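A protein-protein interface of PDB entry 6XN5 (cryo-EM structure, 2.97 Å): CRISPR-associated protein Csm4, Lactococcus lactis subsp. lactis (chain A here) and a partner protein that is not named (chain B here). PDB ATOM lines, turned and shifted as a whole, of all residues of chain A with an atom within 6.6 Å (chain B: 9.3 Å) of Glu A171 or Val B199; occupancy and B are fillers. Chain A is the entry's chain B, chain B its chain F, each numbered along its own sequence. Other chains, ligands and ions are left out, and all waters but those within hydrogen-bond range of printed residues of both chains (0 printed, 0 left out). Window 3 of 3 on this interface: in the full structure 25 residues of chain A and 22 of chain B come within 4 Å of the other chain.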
ATOM      1  N   LEU A  35      15.141 -18.060 -33.946  1.00  0.00           N
ATOM      2  CA  LEU A  35      13.723 -18.137 -33.625  1.00  0.00           C
ATOM      3  C   LEU A  35      13.255 -19.576 -33.478  1.00  0.00           C
ATOM      4  O   LEU A  35      12.368 -19.851 -32.672  1.00  0.00           O
ATOM      5  CB  LEU A  35      12.900 -17.424 -34.687  1.00  0.00           C
ATOM      6  CG  LEU A  35      13.017 -15.908 -34.760  1.00  0.00           C
ATOM      7  CD1 LEU A  35      11.991 -15.405 -35.726  1.00  0.00           C
ATOM      8  CD2 LEU A  35      12.839 -15.277 -33.414  1.00  0.00           C
ATOM      9  N   GLU A  38      14.315 -20.577 -30.057  1.00  0.00           N
ATOM     10  CA  GLU A  38      13.377 -20.028 -29.089  1.00  0.00           C
ATOM     11  C   GLU A  38      11.996 -20.652 -29.180  1.00  0.00           C
ATOM     12  O   GLU A  38      11.244 -20.589 -28.206  1.00  0.00           O
ATOM     13  CB  GLU A  38      13.287 -18.517 -29.245  1.00  0.00           C
ATOM     14  CG  GLU A  38      14.587 -17.856 -28.885  1.00  0.00           C
ATOM     15  CD  GLU A  38      14.920 -18.000 -27.409  1.00  0.00           C
ATOM     16  OE1 GLU A  38      13.991 -18.044 -26.574  1.00  0.00           O
ATOM     17  OE2 GLU A  38      16.117 -18.128 -27.089  1.00  0.00           O
ATOM     18  N   LEU A 166       5.568 -14.777 -34.228  1.00  0.00           N
ATOM     19  CA  LEU A 166       6.824 -14.126 -34.582  1.00  0.00           C
ATOM     20  C   LEU A 166       7.225 -13.094 -33.541  1.00  0.00           C
ATOM     21  O   LEU A 166       8.397 -13.006 -33.169  1.00  0.00           O
ATOM     22  CB  LEU A 166       6.691 -13.476 -35.954  1.00  0.00           C
ATOM     23  CG  LEU A 166       7.818 -12.568 -36.430  1.00  0.00           C
ATOM     24  CD1 LEU A 166       9.068 -13.363 -36.690  1.00  0.00           C
ATOM     25  CD2 LEU A 166       7.386 -11.826 -37.672  1.00  0.00           C
ATOM     26  N   GLU A 167       6.259 -12.331 -33.029  1.00  0.00           N
ATOM     27  CA  GLU A 167       6.566 -11.329 -32.015  1.00  0.00           C
ATOM     28  C   GLU A 167       6.919 -11.970 -30.680  1.00  0.00           C
ATOM     29  O   GLU A 167       7.809 -11.482 -29.973  1.00  0.00           O
ATOM     30  CB  GLU A 167       5.393 -10.371 -31.854  1.00  0.00           C
ATOM     31  CG  GLU A 167       4.955  -9.738 -33.148  1.00  0.00           C
ATOM     32  CD  GLU A 167       4.319  -8.392 -32.930  1.00  0.00           C
ATOM     33  OE1 GLU A 167       4.840  -7.627 -32.092  1.00  0.00           O
ATOM     34  OE2 GLU A 167       3.303  -8.099 -33.592  1.00  0.00           O
ATOM     35  N   GLU A 168       6.239 -13.065 -30.321  1.00  0.00           N
ATOM     36  CA  GLU A 168       6.576 -13.785 -29.094  1.00  0.00           C
ATOM     37  C   GLU A 168       7.979 -14.379 -29.164  1.00  0.00           C
ATOM     38  O   GLU A 168       8.761 -14.289 -28.208  1.00  0.00           O
ATOM     39  CB  GLU A 168       5.549 -14.881 -28.840  1.00  0.00           C
ATOM     40  CG  GLU A 168       5.734 -15.586 -27.519  1.00  0.00           C
ATOM     41  CD  GLU A 168       4.851 -16.800 -27.386  1.00  0.00           C
ATOM     42  OE1 GLU A 168       4.804 -17.384 -26.285  1.00  0.00           O
ATOM     43  OE2 GLU A 168       4.203 -17.172 -28.385  1.00  0.00           O
ATOM     44  N   LEU A 169       8.322 -14.966 -30.309  1.00  0.00           N
ATOM     45  CA  LEU A 169       9.648 -15.536 -30.497  1.00  0.00           C
ATOM     46  C   LEU A 169      10.723 -14.463 -30.554  1.00  0.00           C
ATOM     47  O   LEU A 169      11.840 -14.685 -30.078  1.00  0.00           O
ATOM     48  CB  LEU A 169       9.660 -16.375 -31.767  1.00  0.00           C
ATOM     49  CG  LEU A 169       9.547 -17.887 -31.643  1.00  0.00           C
ATOM     50  CD1 LEU A 169       8.371 -18.298 -30.813  1.00  0.00           C
ATOM     51  CD2 LEU A 169       9.389 -18.432 -33.020  1.00  0.00           C
ATOM     52  N   LEU A 170      10.408 -13.296 -31.122  1.00  0.00           N
ATOM     53  CA  LEU A 170      11.354 -12.189 -31.120  1.00  0.00           C
ATOM     54  C   LEU A 170      11.597 -11.674 -29.714  1.00  0.00           C
ATOM     55  O   LEU A 170      12.736 -11.357 -29.355  1.00  0.00           O
ATOM     56  CB  LEU A 170      10.846 -11.052 -31.994  1.00  0.00           C
ATOM     57  CG  LEU A 170      11.087 -11.134 -33.488  1.00  0.00           C
ATOM     58  CD1 LEU A 170      10.134 -10.179 -34.153  1.00  0.00           C
ATOM     59  CD2 LEU A 170      12.524 -10.807 -33.810  1.00  0.00           C
ATOM     60  N   GLU A 171      10.541 -11.585 -28.908  1.00  0.00           N
ATOM     61  CA  GLU A 171      10.704 -11.092 -27.549  1.00  0.00           C
ATOM     62  C   GLU A 171      11.475 -12.094 -26.701  1.00  0.00           C
ATOM     63  O   GLU A 171      12.248 -11.708 -25.820  1.00  0.00           O
ATOM     64  CB  GLU A 171       9.339 -10.793 -26.942  1.00  0.00           C
ATOM     65  CG  GLU A 171       9.408 -10.198 -25.564  1.00  0.00           C
ATOM     66  CD  GLU A 171       8.049  -9.865 -25.000  1.00  0.00           C
ATOM     67  OE1 GLU A 171       7.042 -10.123 -25.688  1.00  0.00           O
ATOM     68  OE2 GLU A 171       7.990  -9.353 -23.863  1.00  0.00           O
ATOM     69  N   ASN A 172      11.312 -13.389 -26.978  1.00  0.00           N
ATOM     70  CA  ASN A 172      12.108 -14.385 -26.266  1.00  0.00           C
ATOM     71  C   ASN A 172      13.561 -14.381 -26.727  1.00  0.00           C
ATOM     72  O   ASN A 172      14.468 -14.636 -25.932  1.00  0.00           O
ATOM     73  CB  ASN A 172      11.489 -15.767 -26.432  1.00  0.00           C
ATOM     74  CG  ASN A 172      10.359 -16.006 -25.469  1.00  0.00           C
ATOM     75  OD1 ASN A 172      10.526 -16.667 -24.449  1.00  0.00           O
ATOM     76  ND2 ASN A 172       9.199 -15.450 -25.777  1.00  0.00           N
ATOM     77  N   LEU A 173      13.805 -14.096 -28.008  1.00  0.00           N
ATOM     78  CA  LEU A 173      15.168 -13.973 -28.512  1.00  0.00           C
ATOM     79  C   LEU A 173      15.853 -12.713 -28.005  1.00  0.00           C
ATOM     80  O   LEU A 173      17.086 -12.679 -27.923  1.00  0.00           O
ATOM     81  CB  LEU A 173      15.133 -14.004 -30.043  1.00  0.00           C
ATOM     82  CG  LEU A 173      16.374 -13.709 -30.874  1.00  0.00           C
ATOM     83  CD1 LEU A 173      17.414 -14.738 -30.567  1.00  0.00           C
ATOM     84  CD2 LEU A 173      16.056 -13.702 -32.345  1.00  0.00           C
ATOM     85  N   GLN A 174      15.068 -11.694 -27.644  1.00  0.00           N
ATOM     86  CA  GLN A 174      15.608 -10.440 -27.124  1.00  0.00           C
ATOM     87  C   GLN A 174      16.402 -10.649 -25.844  1.00  0.00           C
ATOM     88  O   GLN A 174      17.472 -10.058 -25.669  1.00  0.00           O
ATOM     89  CB  GLN A 174      14.461  -9.467 -26.875  1.00  0.00           C
ATOM     90  CG  GLN A 174      14.868  -8.104 -26.419  1.00  0.00           C
ATOM     91  CD  GLN A 174      13.683  -7.190 -26.252  1.00  0.00           C
ATOM     92  OE1 GLN A 174      12.543  -7.598 -26.448  1.00  0.00           O
ATOM     93  NE2 GLN A 174      13.941  -5.950 -25.877  1.00  0.00           N
ATOM     94  N   TYR A 175      15.910 -11.499 -24.948  1.00  0.00           N
ATOM     95  CA  TYR A 175      16.577 -11.773 -23.686  1.00  0.00           C
ATOM     96  C   TYR A 175      17.415 -13.035 -23.729  1.00  0.00           C
ATOM     97  O   TYR A 175      17.657 -13.640 -22.685  1.00  0.00           O
ATOM     98  CB  TYR A 175      15.556 -11.866 -22.562  1.00  0.00           C
ATOM     99  CG  TYR A 175      14.806 -10.584 -22.348  1.00  0.00           C
ATOM    100  CD1 TYR A 175      15.363  -9.555 -21.609  1.00  0.00           C
ATOM    101  CD2 TYR A 175      13.550 -10.392 -22.900  1.00  0.00           C
ATOM    102  CE1 TYR A 175      14.687  -8.377 -21.417  1.00  0.00           C
ATOM    103  CE2 TYR A 175      12.865  -9.217 -22.713  1.00  0.00           C
ATOM    104  CZ  TYR A 175      13.439  -8.214 -21.972  1.00  0.00           C
ATOM    105  OH  TYR A 175      12.758  -7.035 -21.780  1.00  0.00           O
ATOM    106  N   SER A 176      17.854 -13.451 -24.910  1.00  0.00           N
ATOM    107  CA  SER A 176      18.664 -14.648 -25.084  1.00  0.00           C
ATOM    108  C   SER A 176      19.937 -14.410 -25.863  1.00  0.00           C
ATOM    109  O   SER A 176      20.939 -15.067 -25.601  1.00  0.00           O
ATOM    110  CB  SER A 176      17.857 -15.727 -25.794  1.00  0.00           C
ATOM    111  OG  SER A 176      18.563 -16.948 -25.816  1.00  0.00           O
ATOM    112  N   PHE A 191      14.223  -4.735 -29.684  1.00  0.00           N
ATOM    113  CA  PHE A 191      13.577  -4.718 -30.984  1.00  0.00           C
ATOM    114  C   PHE A 191      12.315  -3.869 -30.928  1.00  0.00           C
ATOM    115  O   PHE A 191      11.718  -3.666 -29.869  1.00  0.00           O
ATOM    116  CB  PHE A 191      13.253  -6.143 -31.448  1.00  0.00           C
ATOM    117  CG  PHE A 191      11.971  -6.688 -30.897  1.00  0.00           C
ATOM    118  CD1 PHE A 191      11.851  -6.997 -29.559  1.00  0.00           C
ATOM    119  CD2 PHE A 191      10.891  -6.911 -31.729  1.00  0.00           C
ATOM    120  CE1 PHE A 191      10.675  -7.501 -29.061  1.00  0.00           C
ATOM    121  CE2 PHE A 191       9.714  -7.413 -31.233  1.00  0.00           C
ATOM    122  CZ  PHE A 191       9.607  -7.708 -29.900  1.00  0.00           C
ATOM    123  N   MET B   1       9.347 -17.487 -17.928  1.00  0.00           N
ATOM    124  CA  MET B   1      10.272 -18.587 -18.148  1.00  0.00           C
ATOM    125  C   MET B   1      11.583 -18.085 -18.720  1.00  0.00           C
ATOM    126  O   MET B   1      12.301 -18.819 -19.386  1.00  0.00           O
ATOM    127  CB  MET B   1       9.650 -19.624 -19.074  1.00  0.00           C
ATOM    128  CG  MET B   1       8.426 -20.336 -18.502  1.00  0.00           C
ATOM    129  SD  MET B   1       8.716 -21.294 -16.994  1.00  0.00           S
ATOM    130  CE  MET B   1       8.051 -20.218 -15.721  1.00  0.00           C
ATOM    131  N   LYS B   2      11.874 -16.817 -18.457  1.00  0.00           N
ATOM    132  CA  LYS B   2      13.159 -16.221 -18.782  1.00  0.00           C
ATOM    133  C   LYS B   2      13.360 -15.047 -17.844  1.00  0.00           C
ATOM    134  O   LYS B   2      12.554 -14.117 -17.840  1.00  0.00           O
ATOM    135  CB  LYS B   2      13.214 -15.776 -20.239  1.00  0.00           C
ATOM    136  CG  LYS B   2      14.591 -15.506 -20.759  1.00  0.00           C
ATOM    137  CD  LYS B   2      14.559 -15.483 -22.262  1.00  0.00           C
ATOM    138  CE  LYS B   2      14.685 -16.871 -22.831  1.00  0.00           C
ATOM    139  NZ  LYS B   2      16.103 -17.279 -22.867  1.00  0.00           N
ATOM    140  N   LEU B   3      14.422 -15.096 -17.052  1.00  0.00           N
ATOM    141  CA  LEU B   3      14.566 -14.240 -15.889  1.00  0.00           C
ATOM    142  C   LEU B   3      15.736 -13.291 -16.077  1.00  0.00           C
ATOM    143  O   LEU B   3      16.682 -13.582 -16.807  1.00  0.00           O
ATOM    144  CB  LEU B   3      14.775 -15.069 -14.621  1.00  0.00           C
ATOM    145  CG  LEU B   3      13.560 -15.545 -13.838  1.00  0.00           C
ATOM    146  CD1 LEU B   3      12.745 -16.567 -14.586  1.00  0.00           C
ATOM    147  CD2 LEU B   3      14.046 -16.138 -12.565  1.00  0.00           C
ATOM    148  N   VAL B   4      15.657 -12.147 -15.405  1.00  0.00           N
ATOM    149  CA  VAL B   4      16.689 -11.122 -15.446  1.00  0.00           C
ATOM    150  C   VAL B   4      17.173 -10.894 -14.028  1.00  0.00           C
ATOM    151  O   VAL B   4      16.363 -10.655 -13.129  1.00  0.00           O
ATOM    152  CB  VAL B   4      16.155  -9.801 -16.034  1.00  0.00           C
ATOM    153  CG1 VAL B   4      17.212  -8.724 -15.976  1.00  0.00           C
ATOM    154  CG2 VAL B   4      15.666 -10.000 -17.438  1.00  0.00           C
ATOM    155  N   PHE B 149      20.956 -12.854 -17.780  1.00  0.00           N
ATOM    156  CA  PHE B 149      19.676 -13.445 -18.130  1.00  0.00           C
ATOM    157  C   PHE B 149      19.686 -14.936 -17.836  1.00  0.00           C
ATOM    158  O   PHE B 149      20.605 -15.653 -18.239  1.00  0.00           O
ATOM    159  CB  PHE B 149      19.345 -13.193 -19.595  1.00  0.00           C
ATOM    160  CG  PHE B 149      19.336 -11.748 -19.965  1.00  0.00           C
ATOM    161  CD1 PHE B 149      18.706 -10.826 -19.165  1.00  0.00           C
ATOM    162  CD2 PHE B 149      19.969 -11.311 -21.110  1.00  0.00           C
ATOM    163  CE1 PHE B 149      18.697  -9.498 -19.504  1.00  0.00           C
ATOM    164  CE2 PHE B 149      19.968  -9.986 -21.451  1.00  0.00           C
ATOM    165  CZ  PHE B 149      19.329  -9.078 -20.648  1.00  0.00           C
ATOM    166  N   TYR B 150      18.660 -15.392 -17.137  1.00  0.00           N
ATOM    167  CA  TYR B 150      18.473 -16.787 -16.773  1.00  0.00           C
ATOM    168  C   TYR B 150      17.257 -17.295 -17.531  1.00  0.00           C
ATOM    169  O   TYR B 150      16.208 -16.647 -17.508  1.00  0.00           O
ATOM    170  CB  TYR B 150      18.269 -16.891 -15.264  1.00  0.00           C
ATOM    171  CG  TYR B 150      18.058 -18.267 -14.704  1.00  0.00           C
ATOM    172  CD1 TYR B 150      19.131 -19.062 -14.356  1.00  0.00           C
ATOM    173  CD2 TYR B 150      16.785 -18.755 -14.488  1.00  0.00           C
ATOM    174  CE1 TYR B 150      18.940 -20.310 -13.828  1.00  0.00           C
ATOM    175  CE2 TYR B 150      16.587 -20.002 -13.965  1.00  0.00           C
ATOM    176  CZ  TYR B 150      17.665 -20.773 -13.635  1.00  0.00           C
ATOM    177  OH  TYR B 150      17.467 -22.022 -13.109  1.00  0.00           O
ATOM    178  N   ASN B 151      17.385 -18.427 -18.219  1.00  0.00           N
ATOM    179  CA  ASN B 151      16.210 -19.047 -18.817  1.00  0.00           C
ATOM    180  C   ASN B 151      15.812 -20.283 -18.026  1.00  0.00           C
ATOM    181  O   ASN B 151      16.657 -21.051 -17.566  1.00  0.00           O
ATOM    182  CB  ASN B 151      16.397 -19.401 -20.295  1.00  0.00           C
ATOM    183  CG  ASN B 151      17.468 -20.409 -20.528  1.00  0.00           C
ATOM    184  OD1 ASN B 151      18.398 -20.512 -19.751  1.00  0.00           O
ATOM    185  ND2 ASN B 151      17.348 -21.166 -21.608  1.00  0.00           N
ATOM    186  N   LEU B 152      14.514 -20.461 -17.878  1.00  0.00           N
ATOM    187  CA  LEU B 152      13.946 -21.381 -16.912  1.00  0.00           C
ATOM    188  C   LEU B 152      13.443 -22.619 -17.643  1.00  0.00           C
ATOM    189  O   LEU B 152      12.286 -22.675 -18.068  1.00  0.00           O
ATOM    190  CB  LEU B 152      12.846 -20.669 -16.130  1.00  0.00           C
ATOM    191  CG  LEU B 152      12.132 -21.366 -14.985  1.00  0.00           C
ATOM    192  CD1 LEU B 152      13.121 -22.108 -14.164  1.00  0.00           C
ATOM    193  CD2 LEU B 152      11.470 -20.310 -14.138  1.00  0.00           C
ATOM    194  N   ILE B 196      14.006  -9.892 -11.715  1.00  0.00           N
ATOM    195  CA  ILE B 196      12.715  -9.598 -12.326  1.00  0.00           C
ATOM    196  C   ILE B 196      12.532 -10.541 -13.511  1.00  0.00           C
ATOM    197  O   ILE B 196      13.493 -10.850 -14.222  1.00  0.00           O
ATOM    198  CB  ILE B 196      12.595  -8.109 -12.730  1.00  0.00           C
ATOM    199  CG1 ILE B 196      11.175  -7.769 -13.187  1.00  0.00           C
ATOM    200  CG2 ILE B 196      13.637  -7.688 -13.760  1.00  0.00           C
ATOM    201  N   THR B 197      11.323 -11.064 -13.674  1.00  0.00           N
ATOM    202  CA  THR B 197      11.056 -11.987 -14.765  1.00  0.00           C
ATOM    203  C   THR B 197      10.793 -11.213 -16.050  1.00  0.00           C
ATOM    204  O   THR B 197      10.116 -10.181 -16.042  1.00  0.00           O
ATOM    205  CB  THR B 197       9.896 -12.922 -14.405  1.00  0.00           C
ATOM    206  OG1 THR B 197       9.651 -13.830 -15.483  1.00  0.00           O
ATOM    207  CG2 THR B 197       8.625 -12.176 -14.040  1.00  0.00           C
ATOM    208  N   ALA B 198      11.383 -11.677 -17.151  1.00  0.00           N
ATOM    209  CA  ALA B 198      11.312 -10.932 -18.403  1.00  0.00           C
ATOM    210  C   ALA B 198      10.101 -11.339 -19.233  1.00  0.00           C
ATOM    211  O   ALA B 198       9.251 -10.503 -19.550  1.00  0.00           O
ATOM    212  CB  ALA B 198      12.597 -11.126 -19.209  1.00  0.00           C
ATOM    213  N   VAL B 199      10.023 -12.612 -19.615  1.00  0.00           N
ATOM    214  CA  VAL B 199       8.864 -13.154 -20.314  1.00  0.00           C
ATOM    215  C   VAL B 199       8.401 -14.406 -19.588  1.00  0.00           C
ATOM    216  O   VAL B 199       9.218 -15.167 -19.061  1.00  0.00           O
ATOM    217  CB  VAL B 199       9.146 -13.447 -21.803  1.00  0.00           C
ATOM    218  CG1 VAL B 199       9.457 -12.182 -22.528  1.00  0.00           C
ATOM    219  CG2 VAL B 199      10.302 -14.390 -21.984  1.00  0.00           C
ATOM    220  N   GLY B 200       7.091 -14.580 -19.501  1.00  0.00           N
ATOM    221  CA  GLY B 200       6.550 -15.752 -18.853  1.00  0.00           C
ATOM    222  C   GLY B 200       6.395 -15.485 -17.376  1.00  0.00           C
ATOM    223  O   GLY B 200       7.396 -15.309 -16.678  1.00  0.00           O
ATOM    224  N   ASN B 201       5.162 -15.445 -16.884  1.00  0.00           N
ATOM    225  CA  ASN B 201       4.933 -15.101 -15.490  1.00  0.00           C
ATOM    226  C   ASN B 201       5.331 -16.272 -14.606  1.00  0.00           C
ATOM    227  O   ASN B 201       4.872 -17.400 -14.810  1.00  0.00           O
ATOM    228  CB  ASN B 201       3.474 -14.721 -15.269  1.00  0.00           C
ATOM    229  CG  ASN B 201       3.299 -13.717 -14.149  1.00  0.00           C
ATOM    230  OD1 ASN B 201       4.257 -13.067 -13.730  1.00  0.00           O
ATOM    231  ND2 ASN B 201       2.073 -13.580 -13.659  1.00  0.00           N
ATOM    232  N   PHE B 202       6.202 -16.010 -13.639  1.00  0.00           N
ATOM    233  CA  PHE B 202       6.724 -17.042 -12.759  1.00  0.00           C
ATOM    234  C   PHE B 202       6.096 -16.858 -11.387  1.00  0.00           C
ATOM    235  O   PHE B 202       6.128 -15.758 -10.827  1.00  0.00           O
ATOM    236  CB  PHE B 202       8.248 -16.966 -12.686  1.00  0.00           C
ATOM    237  CG  PHE B 202       8.874 -18.065 -11.892  1.00  0.00           C
ATOM    238  CD1 PHE B 202       8.317 -19.331 -11.870  1.00  0.00           C
ATOM    239  CD2 PHE B 202      10.040 -17.844 -11.196  1.00  0.00           C
ATOM    240  CE1 PHE B 202       8.895 -20.340 -11.143  1.00  0.00           C
ATOM    241  CE2 PHE B 202      10.624 -18.853 -10.480  1.00  0.00           C
ATOM    242  CZ  PHE B 202      10.052 -20.098 -10.446  1.00  0.00           C
ATOM    243  N   ILE B 205       8.521 -15.796  -7.679  1.00  0.00           N
ATOM    244  CA  ILE B 205       9.651 -14.945  -8.004  1.00  0.00           C
ATOM    245  C   ILE B 205      10.225 -14.258  -6.767  1.00  0.00           C
ATOM    246  O   ILE B 205      11.431 -13.980  -6.728  1.00  0.00           O
ATOM    247  CB  ILE B 205       9.260 -13.913  -9.091  1.00  0.00           C
ATOM    248  CG1 ILE B 205      10.473 -13.154  -9.639  1.00  0.00           C
ATOM    249  CG2 ILE B 205       8.187 -12.947  -8.601  1.00  0.00           C
ATOM    250  CD1 ILE B 205      11.422 -14.006 -10.419  1.00  0.00           C
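OE1 of Glu A38 touches CE of Lys B2 (3.98 Å).
Val B199 touches Glu A171.
CD of Lys B2 touches O of Asn A172 (3.8 Å).
Asn A172 touches Val B199.
CD of Lys B2 touches O of Tyr A175 (3.6 Å).
Phe B149 touches Tyr A175.
CB of Ala B198 touches CG of Tyr A175, 3.9 Å away.
CB of Ser A176 touches NZ of Lys B2, 3.7 Å away.
Hydrophobic or aromatic side chains of chain A that line the printed part of chain B: Tyr A175.
Printed residues of chain B that touch a printed residue of chain A: Lys B2, Phe B149, Ala B198 and Val B199.
Hydrophobic or aromatic side chains of chain B that line the printed part of chain A: Phe B149, Ala B198 and Val B199.
Among the printed residues, no Asp or Glu carboxylate lies within 4 Å of a Lys or Arg side-chain nitrogen of the other chain.
Glu A171 touches one residue of chain B.
Asn A172 touches two residues of chain B.
Printed residues of chain B within 4 Å of Tyr A175: Lys B2 (3.6 Å), Phe B149 (3.5 Å) and Ala B198 (3.9 Å).
Of the printed residues of chain A, Phe B149 touches Tyr A175 (3.5 Å).
Ile B196 touches none of the printed residues of chain A.
Printed residues of chain A within 4 Å of Ala B198: Tyr A175.
Asn B201 touches none of the printed residues of chain A.
The nearest residue of chain A that does not touch Val B199 is Tyr A175 (4.5 Å).
The nearest printed residue of chain A that does not touch Lys B2 is Glu A171 (5.7 Å).
O of Glu A168 lies within hydrogen-bond range of ND2 of Asn A172 (2.7 Å).
The side-chain carboxylate (OE2) of Glu A38 lies within hydrogen-bond range of the side-chain hydroxyl (OG) of Ser A176, at 3.0 Å.
The backbone NH (N) of Met B1 sits at hydrogen-bond distance from the backbone carbonyl oxygen (O) of Val B199, at 2.6 Å.
The backbone carbonyl oxygen (O) of Val B199 is in hydrogen-bond range of the backbone NH (N) of Lys B2 (3.2 Å).
The backbone NH of Ala B198 is in hydrogen-bond range of the backbone carbonyl oxygen of Lys B2 (2.8 Å).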
